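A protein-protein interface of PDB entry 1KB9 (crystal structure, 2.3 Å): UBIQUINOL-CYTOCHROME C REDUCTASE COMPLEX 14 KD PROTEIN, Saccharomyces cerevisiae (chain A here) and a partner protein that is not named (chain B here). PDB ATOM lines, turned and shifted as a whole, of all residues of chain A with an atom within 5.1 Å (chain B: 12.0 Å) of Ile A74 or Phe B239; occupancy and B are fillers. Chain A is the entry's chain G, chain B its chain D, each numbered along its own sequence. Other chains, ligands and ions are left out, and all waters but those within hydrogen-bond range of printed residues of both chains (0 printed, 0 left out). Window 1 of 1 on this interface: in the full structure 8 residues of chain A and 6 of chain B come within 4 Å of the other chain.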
ATOM      1  N   ARG A  69      -4.586  38.458  21.462  1.00  0.00           N
ATOM      2  CA  ARG A  69      -3.533  38.071  20.526  1.00  0.00           C
ATOM      3  C   ARG A  69      -3.011  36.688  20.938  1.00  0.00           C
ATOM      4  O   ARG A  69      -2.855  35.800  20.096  1.00  0.00           O
ATOM      5  CB  ARG A  69      -2.379  39.098  20.517  1.00  0.00           C
ATOM      6  CG  ARG A  69      -1.440  38.936  19.320  1.00  0.00           C
ATOM      7  CD  ARG A  69      -0.173  39.790  19.382  1.00  0.00           C
ATOM      8  NE  ARG A  69       0.690  39.263  20.416  1.00  0.00           N
ATOM      9  CZ  ARG A  69       1.933  38.836  20.251  1.00  0.00           C
ATOM     10  NH1 ARG A  69       2.561  38.360  21.307  1.00  0.00           N
ATOM     11  NH2 ARG A  69       2.566  38.925  19.081  1.00  0.00           N
ATOM     12  N   ALA A  70      -2.833  36.491  22.244  1.00  0.00           N
ATOM     13  CA  ALA A  70      -2.331  35.226  22.785  1.00  0.00           C
ATOM     14  C   ALA A  70      -3.225  34.045  22.420  1.00  0.00           C
ATOM     15  O   ALA A  70      -2.735  32.986  22.013  1.00  0.00           O
ATOM     16  CB  ALA A  70      -2.169  35.319  24.303  1.00  0.00           C
ATOM     17  N   TYR A  71      -4.533  34.232  22.565  1.00  0.00           N
ATOM     18  CA  TYR A  71      -5.483  33.176  22.230  1.00  0.00           C
ATOM     19  C   TYR A  71      -5.471  32.860  20.738  1.00  0.00           C
ATOM     20  O   TYR A  71      -5.498  31.693  20.349  1.00  0.00           O
ATOM     21  CB  TYR A  71      -6.910  33.548  22.665  1.00  0.00           C
ATOM     22  CG  TYR A  71      -7.932  32.515  22.255  1.00  0.00           C
ATOM     23  CD1 TYR A  71      -7.840  31.203  22.713  1.00  0.00           C
ATOM     24  CD2 TYR A  71      -8.946  32.826  21.349  1.00  0.00           C
ATOM     25  CE1 TYR A  71      -8.725  30.221  22.274  1.00  0.00           C
ATOM     26  CE2 TYR A  71      -9.841  31.847  20.901  1.00  0.00           C
ATOM     27  CZ  TYR A  71      -9.722  30.548  21.367  1.00  0.00           C
ATOM     28  OH  TYR A  71     -10.581  29.565  20.919  1.00  0.00           O
ATOM     29  N   ARG A  72      -5.444  33.900  19.908  1.00  0.00           N
ATOM     30  CA  ARG A  72      -5.438  33.708  18.461  1.00  0.00           C
ATOM     31  C   ARG A  72      -4.204  32.943  18.000  1.00  0.00           C
ATOM     32  O   ARG A  72      -4.306  32.014  17.192  1.00  0.00           O
ATOM     33  CB  ARG A  72      -5.555  35.048  17.719  1.00  0.00           C
ATOM     34  CG  ARG A  72      -6.898  35.744  17.897  1.00  0.00           C
ATOM     35  CD  ARG A  72      -7.115  36.831  16.852  1.00  0.00           C
ATOM     36  NE  ARG A  72      -6.109  37.891  16.921  1.00  0.00           N
ATOM     37  CZ  ARG A  72      -6.174  38.944  17.729  1.00  0.00           C
ATOM     38  NH1 ARG A  72      -5.203  39.848  17.719  1.00  0.00           N
ATOM     39  NH2 ARG A  72      -7.208  39.096  18.541  1.00  0.00           N
ATOM     40  N   ILE A  73      -3.048  33.311  18.548  1.00  0.00           N
ATOM     41  CA  ILE A  73      -1.786  32.654  18.215  1.00  0.00           C
ATOM     42  C   ILE A  73      -1.784  31.181  18.656  1.00  0.00           C
ATOM     43  O   ILE A  73      -1.425  30.284  17.881  1.00  0.00           O
ATOM     44  CB  ILE A  73      -0.599  33.422  18.824  1.00  0.00           C
ATOM     45  CG1 ILE A  73      -0.440  34.762  18.094  1.00  0.00           C
ATOM     46  CG2 ILE A  73       0.689  32.589  18.743  1.00  0.00           C
ATOM     47  CD1 ILE A  73       0.547  35.711  18.737  1.00  0.00           C
ATOM     48  N   ILE A  74      -2.235  30.926  19.880  1.00  0.00           N
ATOM     49  CA  ILE A  74      -2.287  29.555  20.376  1.00  0.00           C
ATOM     50  C   ILE A  74      -3.269  28.732  19.551  1.00  0.00           C
ATOM     51  O   ILE A  74      -2.960  27.615  19.136  1.00  0.00           O
ATOM     52  CB  ILE A  74      -2.658  29.495  21.872  1.00  0.00           C
ATOM     53  CG1 ILE A  74      -1.545  30.129  22.705  1.00  0.00           C
ATOM     54  CG2 ILE A  74      -2.860  28.059  22.307  1.00  0.00           C
ATOM     55  CD1 ILE A  74      -1.873  30.263  24.171  1.00  0.00           C
ATOM     56  N   ARG A  75      -4.430  29.309  19.265  1.00  0.00           N
ATOM     57  CA  ARG A  75      -5.452  28.619  18.471  1.00  0.00           C
ATOM     58  C   ARG A  75      -4.929  28.299  17.063  1.00  0.00           C
ATOM     59  O   ARG A  75      -5.212  27.235  16.514  1.00  0.00           O
ATOM     60  CB  ARG A  75      -6.726  29.467  18.404  1.00  0.00           C
ATOM     61  CG  ARG A  75      -7.885  28.826  17.669  1.00  0.00           C
ATOM     62  CD  ARG A  75      -8.506  29.835  16.714  1.00  0.00           C
ATOM     63  NE  ARG A  75      -9.635  30.578  17.271  1.00  0.00           N
ATOM     64  CZ  ARG A  75      -9.897  31.861  17.030  1.00  0.00           C
ATOM     65  NH1 ARG A  75     -10.965  32.418  17.576  1.00  0.00           N
ATOM     66  NH2 ARG A  75      -9.075  32.604  16.303  1.00  0.00           N
ATOM     67  N   ALA A  76      -4.134  29.205  16.500  1.00  0.00           N
ATOM     68  CA  ALA A  76      -3.563  28.988  15.172  1.00  0.00           C
ATOM     69  C   ALA A  76      -2.565  27.814  15.161  1.00  0.00           C
ATOM     70  O   ALA A  76      -2.574  26.998  14.229  1.00  0.00           O
ATOM     71  CB  ALA A  76      -2.896  30.268  14.660  1.00  0.00           C
ATOM     72  N   HIS A  77      -1.715  27.722  16.188  1.00  0.00           N
ATOM     73  CA  HIS A  77      -0.745  26.629  16.259  1.00  0.00           C
ATOM     74  C   HIS A  77      -1.423  25.270  16.370  1.00  0.00           C
ATOM     75  O   HIS A  77      -1.022  24.316  15.692  1.00  0.00           O
ATOM     76  CB  HIS A  77       0.241  26.823  17.416  1.00  0.00           C
ATOM     77  CG  HIS A  77       1.348  27.787  17.112  1.00  0.00           C
ATOM     78  ND1 HIS A  77       1.471  29.007  17.742  1.00  0.00           N
ATOM     79  CD2 HIS A  77       2.392  27.701  16.254  1.00  0.00           C
ATOM     80  CE1 HIS A  77       2.546  29.629  17.289  1.00  0.00           C
ATOM     81  NE2 HIS A  77       3.122  28.857  16.386  1.00  0.00           N
ATOM     82  N   GLN A  78      -2.458  25.193  17.206  1.00  0.00           N
ATOM     83  CA  GLN A  78      -3.201  23.948  17.400  1.00  0.00           C
ATOM     84  C   GLN A  78      -3.901  23.510  16.116  1.00  0.00           C
ATOM     85  O   GLN A  78      -3.876  22.331  15.758  1.00  0.00           O
ATOM     86  CB  GLN A  78      -4.228  24.103  18.519  1.00  0.00           C
ATOM     87  CG  GLN A  78      -5.062  22.854  18.756  1.00  0.00           C
ATOM     88  CD  GLN A  78      -4.237  21.672  19.236  1.00  0.00           C
ATOM     89  OE1 GLN A  78      -3.244  21.838  19.946  1.00  0.00           O
ATOM     90  NE2 GLN A  78      -4.646  20.472  18.853  1.00  0.00           N
ATOM     91  N   TRP B 231       1.022  11.053  20.411  1.00  0.00           N
ATOM     92  CA  TRP B 231       0.551  12.396  20.080  1.00  0.00           C
ATOM     93  C   TRP B 231      -0.967  12.638  20.235  1.00  0.00           C
ATOM     94  O   TRP B 231      -1.408  13.795  20.188  1.00  0.00           O
ATOM     95  CB  TRP B 231       0.962  12.757  18.642  1.00  0.00           C
ATOM     96  CG  TRP B 231       2.350  13.292  18.504  1.00  0.00           C
ATOM     97  CD1 TRP B 231       3.513  12.579  18.549  1.00  0.00           C
ATOM     98  CD2 TRP B 231       2.725  14.660  18.304  1.00  0.00           C
ATOM     99  NE1 TRP B 231       4.591  13.418  18.392  1.00  0.00           N
ATOM    100  CE2 TRP B 231       4.137  14.701  18.242  1.00  0.00           C
ATOM    101  CE3 TRP B 231       2.006  15.859  18.179  1.00  0.00           C
ATOM    102  CZ2 TRP B 231       4.848  15.899  18.064  1.00  0.00           C
ATOM    103  CZ3 TRP B 231       2.714  17.050  18.004  1.00  0.00           C
ATOM    104  CH2 TRP B 231       4.123  17.058  17.950  1.00  0.00           C
ATOM    105  N   ALA B 232      -1.752  11.574  20.440  1.00  0.00           N
ATOM    106  CA  ALA B 232      -3.219  11.695  20.551  1.00  0.00           C
ATOM    107  C   ALA B 232      -3.738  12.756  21.525  1.00  0.00           C
ATOM    108  O   ALA B 232      -4.711  13.443  21.233  1.00  0.00           O
ATOM    109  CB  ALA B 232      -3.864  10.336  20.843  1.00  0.00           C
ATOM    110  N   GLY B 233      -3.085  12.905  22.668  1.00  0.00           N
ATOM    111  CA  GLY B 233      -3.521  13.911  23.616  1.00  0.00           C
ATOM    112  C   GLY B 233      -3.351  15.328  23.091  1.00  0.00           C
ATOM    113  O   GLY B 233      -4.193  16.194  23.343  1.00  0.00           O
ATOM    114  N   ILE B 234      -2.262  15.565  22.359  1.00  0.00           N
ATOM    115  CA  ILE B 234      -1.959  16.888  21.798  1.00  0.00           C
ATOM    116  C   ILE B 234      -2.834  17.200  20.587  1.00  0.00           C
ATOM    117  O   ILE B 234      -3.391  18.291  20.472  1.00  0.00           O
ATOM    118  CB  ILE B 234      -0.442  16.998  21.411  1.00  0.00           C
ATOM    119  CG1 ILE B 234       0.420  16.972  22.674  1.00  0.00           C
ATOM    120  CG2 ILE B 234      -0.160  18.262  20.612  1.00  0.00           C
ATOM    121  CD1 ILE B 234       0.137  18.098  23.643  1.00  0.00           C
ATOM    122  N   LYS B 235      -2.991  16.216  19.713  1.00  0.00           N
ATOM    123  CA  LYS B 235      -3.784  16.380  18.507  1.00  0.00           C
ATOM    124  C   LYS B 235      -5.257  16.684  18.763  1.00  0.00           C
ATOM    125  O   LYS B 235      -5.858  17.496  18.058  1.00  0.00           O
ATOM    126  CB  LYS B 235      -3.654  15.138  17.628  1.00  0.00           C
ATOM    127  CG  LYS B 235      -2.284  14.954  17.005  1.00  0.00           C
ATOM    128  CD  LYS B 235      -2.137  15.771  15.734  1.00  0.00           C
ATOM    129  CE  LYS B 235      -0.836  15.433  15.016  1.00  0.00           C
ATOM    130  NZ  LYS B 235      -0.734  16.046  13.664  1.00  0.00           N
ATOM    131  N   THR B 236      -5.838  16.043  19.769  1.00  0.00           N
ATOM    132  CA  THR B 236      -7.246  16.259  20.068  1.00  0.00           C
ATOM    133  C   THR B 236      -7.497  17.288  21.162  1.00  0.00           C
ATOM    134  O   THR B 236      -8.630  17.516  21.558  1.00  0.00           O
ATOM    135  CB  THR B 236      -7.943  14.936  20.403  1.00  0.00           C
ATOM    136  OG1 THR B 236      -7.268  14.306  21.498  1.00  0.00           O
ATOM    137  CG2 THR B 236      -7.909  14.009  19.186  1.00  0.00           C
ATOM    138  N   ARG B 237      -6.432  17.928  21.620  1.00  0.00           N
ATOM    139  CA  ARG B 237      -6.496  18.951  22.658  1.00  0.00           C
ATOM    140  C   ARG B 237      -7.454  20.067  22.210  1.00  0.00           C
ATOM    141  O   ARG B 237      -7.548  20.359  21.019  1.00  0.00           O
ATOM    142  CB  ARG B 237      -5.077  19.493  22.874  1.00  0.00           C
ATOM    143  CG  ARG B 237      -4.904  20.552  23.935  1.00  0.00           C
ATOM    144  CD  ARG B 237      -3.413  20.837  24.142  1.00  0.00           C
ATOM    145  NE  ARG B 237      -2.733  21.160  22.886  1.00  0.00           N
ATOM    146  CZ  ARG B 237      -1.609  21.870  22.794  1.00  0.00           C
ATOM    147  NH1 ARG B 237      -1.082  22.118  21.602  1.00  0.00           N
ATOM    148  NH2 ARG B 237      -1.004  22.323  23.887  1.00  0.00           N
ATOM    149  N   LYS B 238      -8.189  20.658  23.153  1.00  0.00           N
ATOM    150  CA  LYS B 238      -9.138  21.728  22.828  1.00  0.00           C
ATOM    151  C   LYS B 238      -9.002  22.948  23.725  1.00  0.00           C
ATOM    152  O   LYS B 238      -8.804  22.825  24.932  1.00  0.00           O
ATOM    153  CB  LYS B 238     -10.579  21.206  22.871  1.00  0.00           C
ATOM    154  CG  LYS B 238     -10.807  20.041  21.919  1.00  0.00           C
ATOM    155  CD  LYS B 238     -12.264  19.757  21.641  1.00  0.00           C
ATOM    156  CE  LYS B 238     -12.380  18.613  20.641  1.00  0.00           C
ATOM    157  NZ  LYS B 238     -13.788  18.353  20.211  1.00  0.00           N
ATOM    158  N   PHE B 239      -9.108  24.128  23.123  1.00  0.00           N
ATOM    159  CA  PHE B 239      -8.994  25.388  23.858  1.00  0.00           C
ATOM    160  C   PHE B 239     -10.313  26.191  23.911  1.00  0.00           C
ATOM    161  O   PHE B 239     -11.184  26.046  23.044  1.00  0.00           O
ATOM    162  CB  PHE B 239      -7.905  26.271  23.227  1.00  0.00           C
ATOM    163  CG  PHE B 239      -6.507  25.729  23.374  1.00  0.00           C
ATOM    164  CD1 PHE B 239      -6.020  24.763  22.494  1.00  0.00           C
ATOM    165  CD2 PHE B 239      -5.673  26.186  24.388  1.00  0.00           C
ATOM    166  CE1 PHE B 239      -4.722  24.257  22.624  1.00  0.00           C
ATOM    167  CE2 PHE B 239      -4.374  25.689  24.529  1.00  0.00           C
ATOM    168  CZ  PHE B 239      -3.901  24.721  23.642  1.00  0.00           C
ATOM    169  N   VAL B 240     -10.461  27.001  24.958  1.00  0.00           N
ATOM    170  CA  VAL B 240     -11.622  27.879  25.125  1.00  0.00           C
ATOM    171  C   VAL B 240     -11.128  29.209  25.689  1.00  0.00           C
ATOM    172  O   VAL B 240     -10.299  29.247  26.592  1.00  0.00           O
ATOM    173  CB  VAL B 240     -12.712  27.307  26.072  1.00  0.00           C
ATOM    174  CG1 VAL B 240     -13.260  26.009  25.537  1.00  0.00           C
ATOM    175  CG2 VAL B 240     -12.173  27.131  27.475  1.00  0.00           C
ATOM    176  N   PHE B 241     -11.631  30.303  25.141  1.00  0.00           N
ATOM    177  CA  PHE B 241     -11.224  31.620  25.600  1.00  0.00           C
ATOM    178  C   PHE B 241     -12.398  32.380  26.229  1.00  0.00           C
ATOM    179  O   PHE B 241     -13.492  32.444  25.663  1.00  0.00           O
ATOM    180  CB  PHE B 241     -10.647  32.402  24.421  1.00  0.00           C
ATOM    181  CG  PHE B 241     -10.158  33.781  24.768  1.00  0.00           C
ATOM    182  CD1 PHE B 241      -9.285  33.987  25.837  1.00  0.00           C
ATOM    183  CD2 PHE B 241     -10.532  34.872  23.991  1.00  0.00           C
ATOM    184  CE1 PHE B 241      -8.786  35.261  26.129  1.00  0.00           C
ATOM    185  CE2 PHE B 241     -10.040  36.154  24.275  1.00  0.00           C
ATOM    186  CZ  PHE B 241      -9.163  36.345  25.346  1.00  0.00           C
ATOM    187  N   ASN B 242     -12.172  32.886  27.436  1.00  0.00           N
ATOM    188  CA  ASN B 242     -13.153  33.680  28.156  1.00  0.00           C
ATOM    189  C   ASN B 242     -12.417  34.969  28.497  1.00  0.00           C
ATOM    190  O   ASN B 242     -11.629  35.011  29.441  1.00  0.00           O
ATOM    191  CB  ASN B 242     -13.616  32.966  29.432  1.00  0.00           C
ATOM    192  CG  ASN B 242     -14.542  31.804  29.143  1.00  0.00           C
ATOM    193  OD1 ASN B 242     -15.471  31.926  28.352  1.00  0.00           O
ATOM    194  ND2 ASN B 242     -14.294  30.671  29.779  1.00  0.00           N
ATOM    195  N   PRO B 243     -12.633  36.029  27.700  1.00  0.00           N
ATOM    196  CA  PRO B 243     -11.981  37.321  27.917  1.00  0.00           C
ATOM    197  C   PRO B 243     -12.066  37.812  29.361  1.00  0.00           C
ATOM    198  O   PRO B 243     -13.153  37.936  29.932  1.00  0.00           O
ATOM    199  CB  PRO B 243     -12.718  38.240  26.949  1.00  0.00           C
ATOM    200  CG  PRO B 243     -13.071  37.320  25.829  1.00  0.00           C
ATOM    201  CD  PRO B 243     -13.553  36.093  26.550  1.00  0.00           C
ATOM    202  N   PRO B 244     -10.904  38.052  29.982  1.00  0.00           N
ATOM    203  CA  PRO B 244     -10.804  38.524  31.365  1.00  0.00           C
ATOM    204  C   PRO B 244     -11.363  39.928  31.529  1.00  0.00           C
ATOM    205  O   PRO B 244     -11.081  40.817  30.720  1.00  0.00           O
ATOM    206  CB  PRO B 244      -9.291  38.529  31.616  1.00  0.00           C
ATOM    207  CG  PRO B 244      -8.769  37.510  30.660  1.00  0.00           C
ATOM    208  CD  PRO B 244      -9.565  37.798  29.425  1.00  0.00           C
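Of the 10 printed residues of chain A, 3 touch a printed residue of chain B.
Hydrophobic or aromatic side chains of chain A within 4 Å of the printed part of chain B: Tyr A71 and Ile A74.
Of the 14 printed residues of chain B, 5 touch a printed residue of chain A.
Printed residues of chain B that touch a printed residue of chain A: Ile B234, Lys B235, Arg B237, Phe B239 and Phe B241.
Hydrophobic or aromatic side chains of chain B within 4 Å of the printed part of chain A: Phe B239 and Phe B241.
Among the printed residues, no Asp or Glu carboxylate lies within 4 Å of a Lys or Arg side-chain nitrogen of the other chain.
OE1 of Gln A78 is in hydrogen-bond range of NH1 of Arg B237, at 2.7 Å.
The backbone carbonyl oxygen (O) of Ile B234 sits at hydrogen-bond distance from the side-chain amide nitrogen (NE2) of Gln A78 (3.0 Å).
The backbone carbonyl oxygen of Lys B235 sits at hydrogen-bond distance from the side-chain amide nitrogen of Gln A78 (3.3 Å).
Of chain B, only Phe B241 (3.5 Å) comes within 4 Å of Tyr A71.
No residue of chain B comes within 4 Å of Ile A73.
Ile A74 touches just one residue of chain B: Phe B239.
No residue of chain B comes within 4 Å of Ala A76.
No residue of chain B comes within 4 Å of His A77.
Gln A78 touches just these residues of chain B: Ile B234, Lys B235, Arg B237 and Phe B239.
Trp B231 touches none of the printed residues of chain A.
Printed residues of chain A within 4 Å of Arg B237: Gln A78 (2.7 Å).
Lys B238 touches none of the printed residues of chain A.
Phe B239 touches just these residues of chain A: Ile A74 and Gln A78.
Of the printed residues of chain A, Phe B241 touches Tyr A71 (3.5 Å).
The nearest residue of chain A that does not touch Phe B239 is Tyr A71 (4.1 Å).
The nearest printed residue of chain A that does not touch Arg B237 is His A77 (6.1 Å).
CB of Phe B241 touches CG of Tyr A71, 3.5 Å away.
Phe B239 touches Ile A74 (CE2 to CG2, 3.6 Å).
OE1 of Gln A78 touches CE1 of Phe B239, 3.9 Å away.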
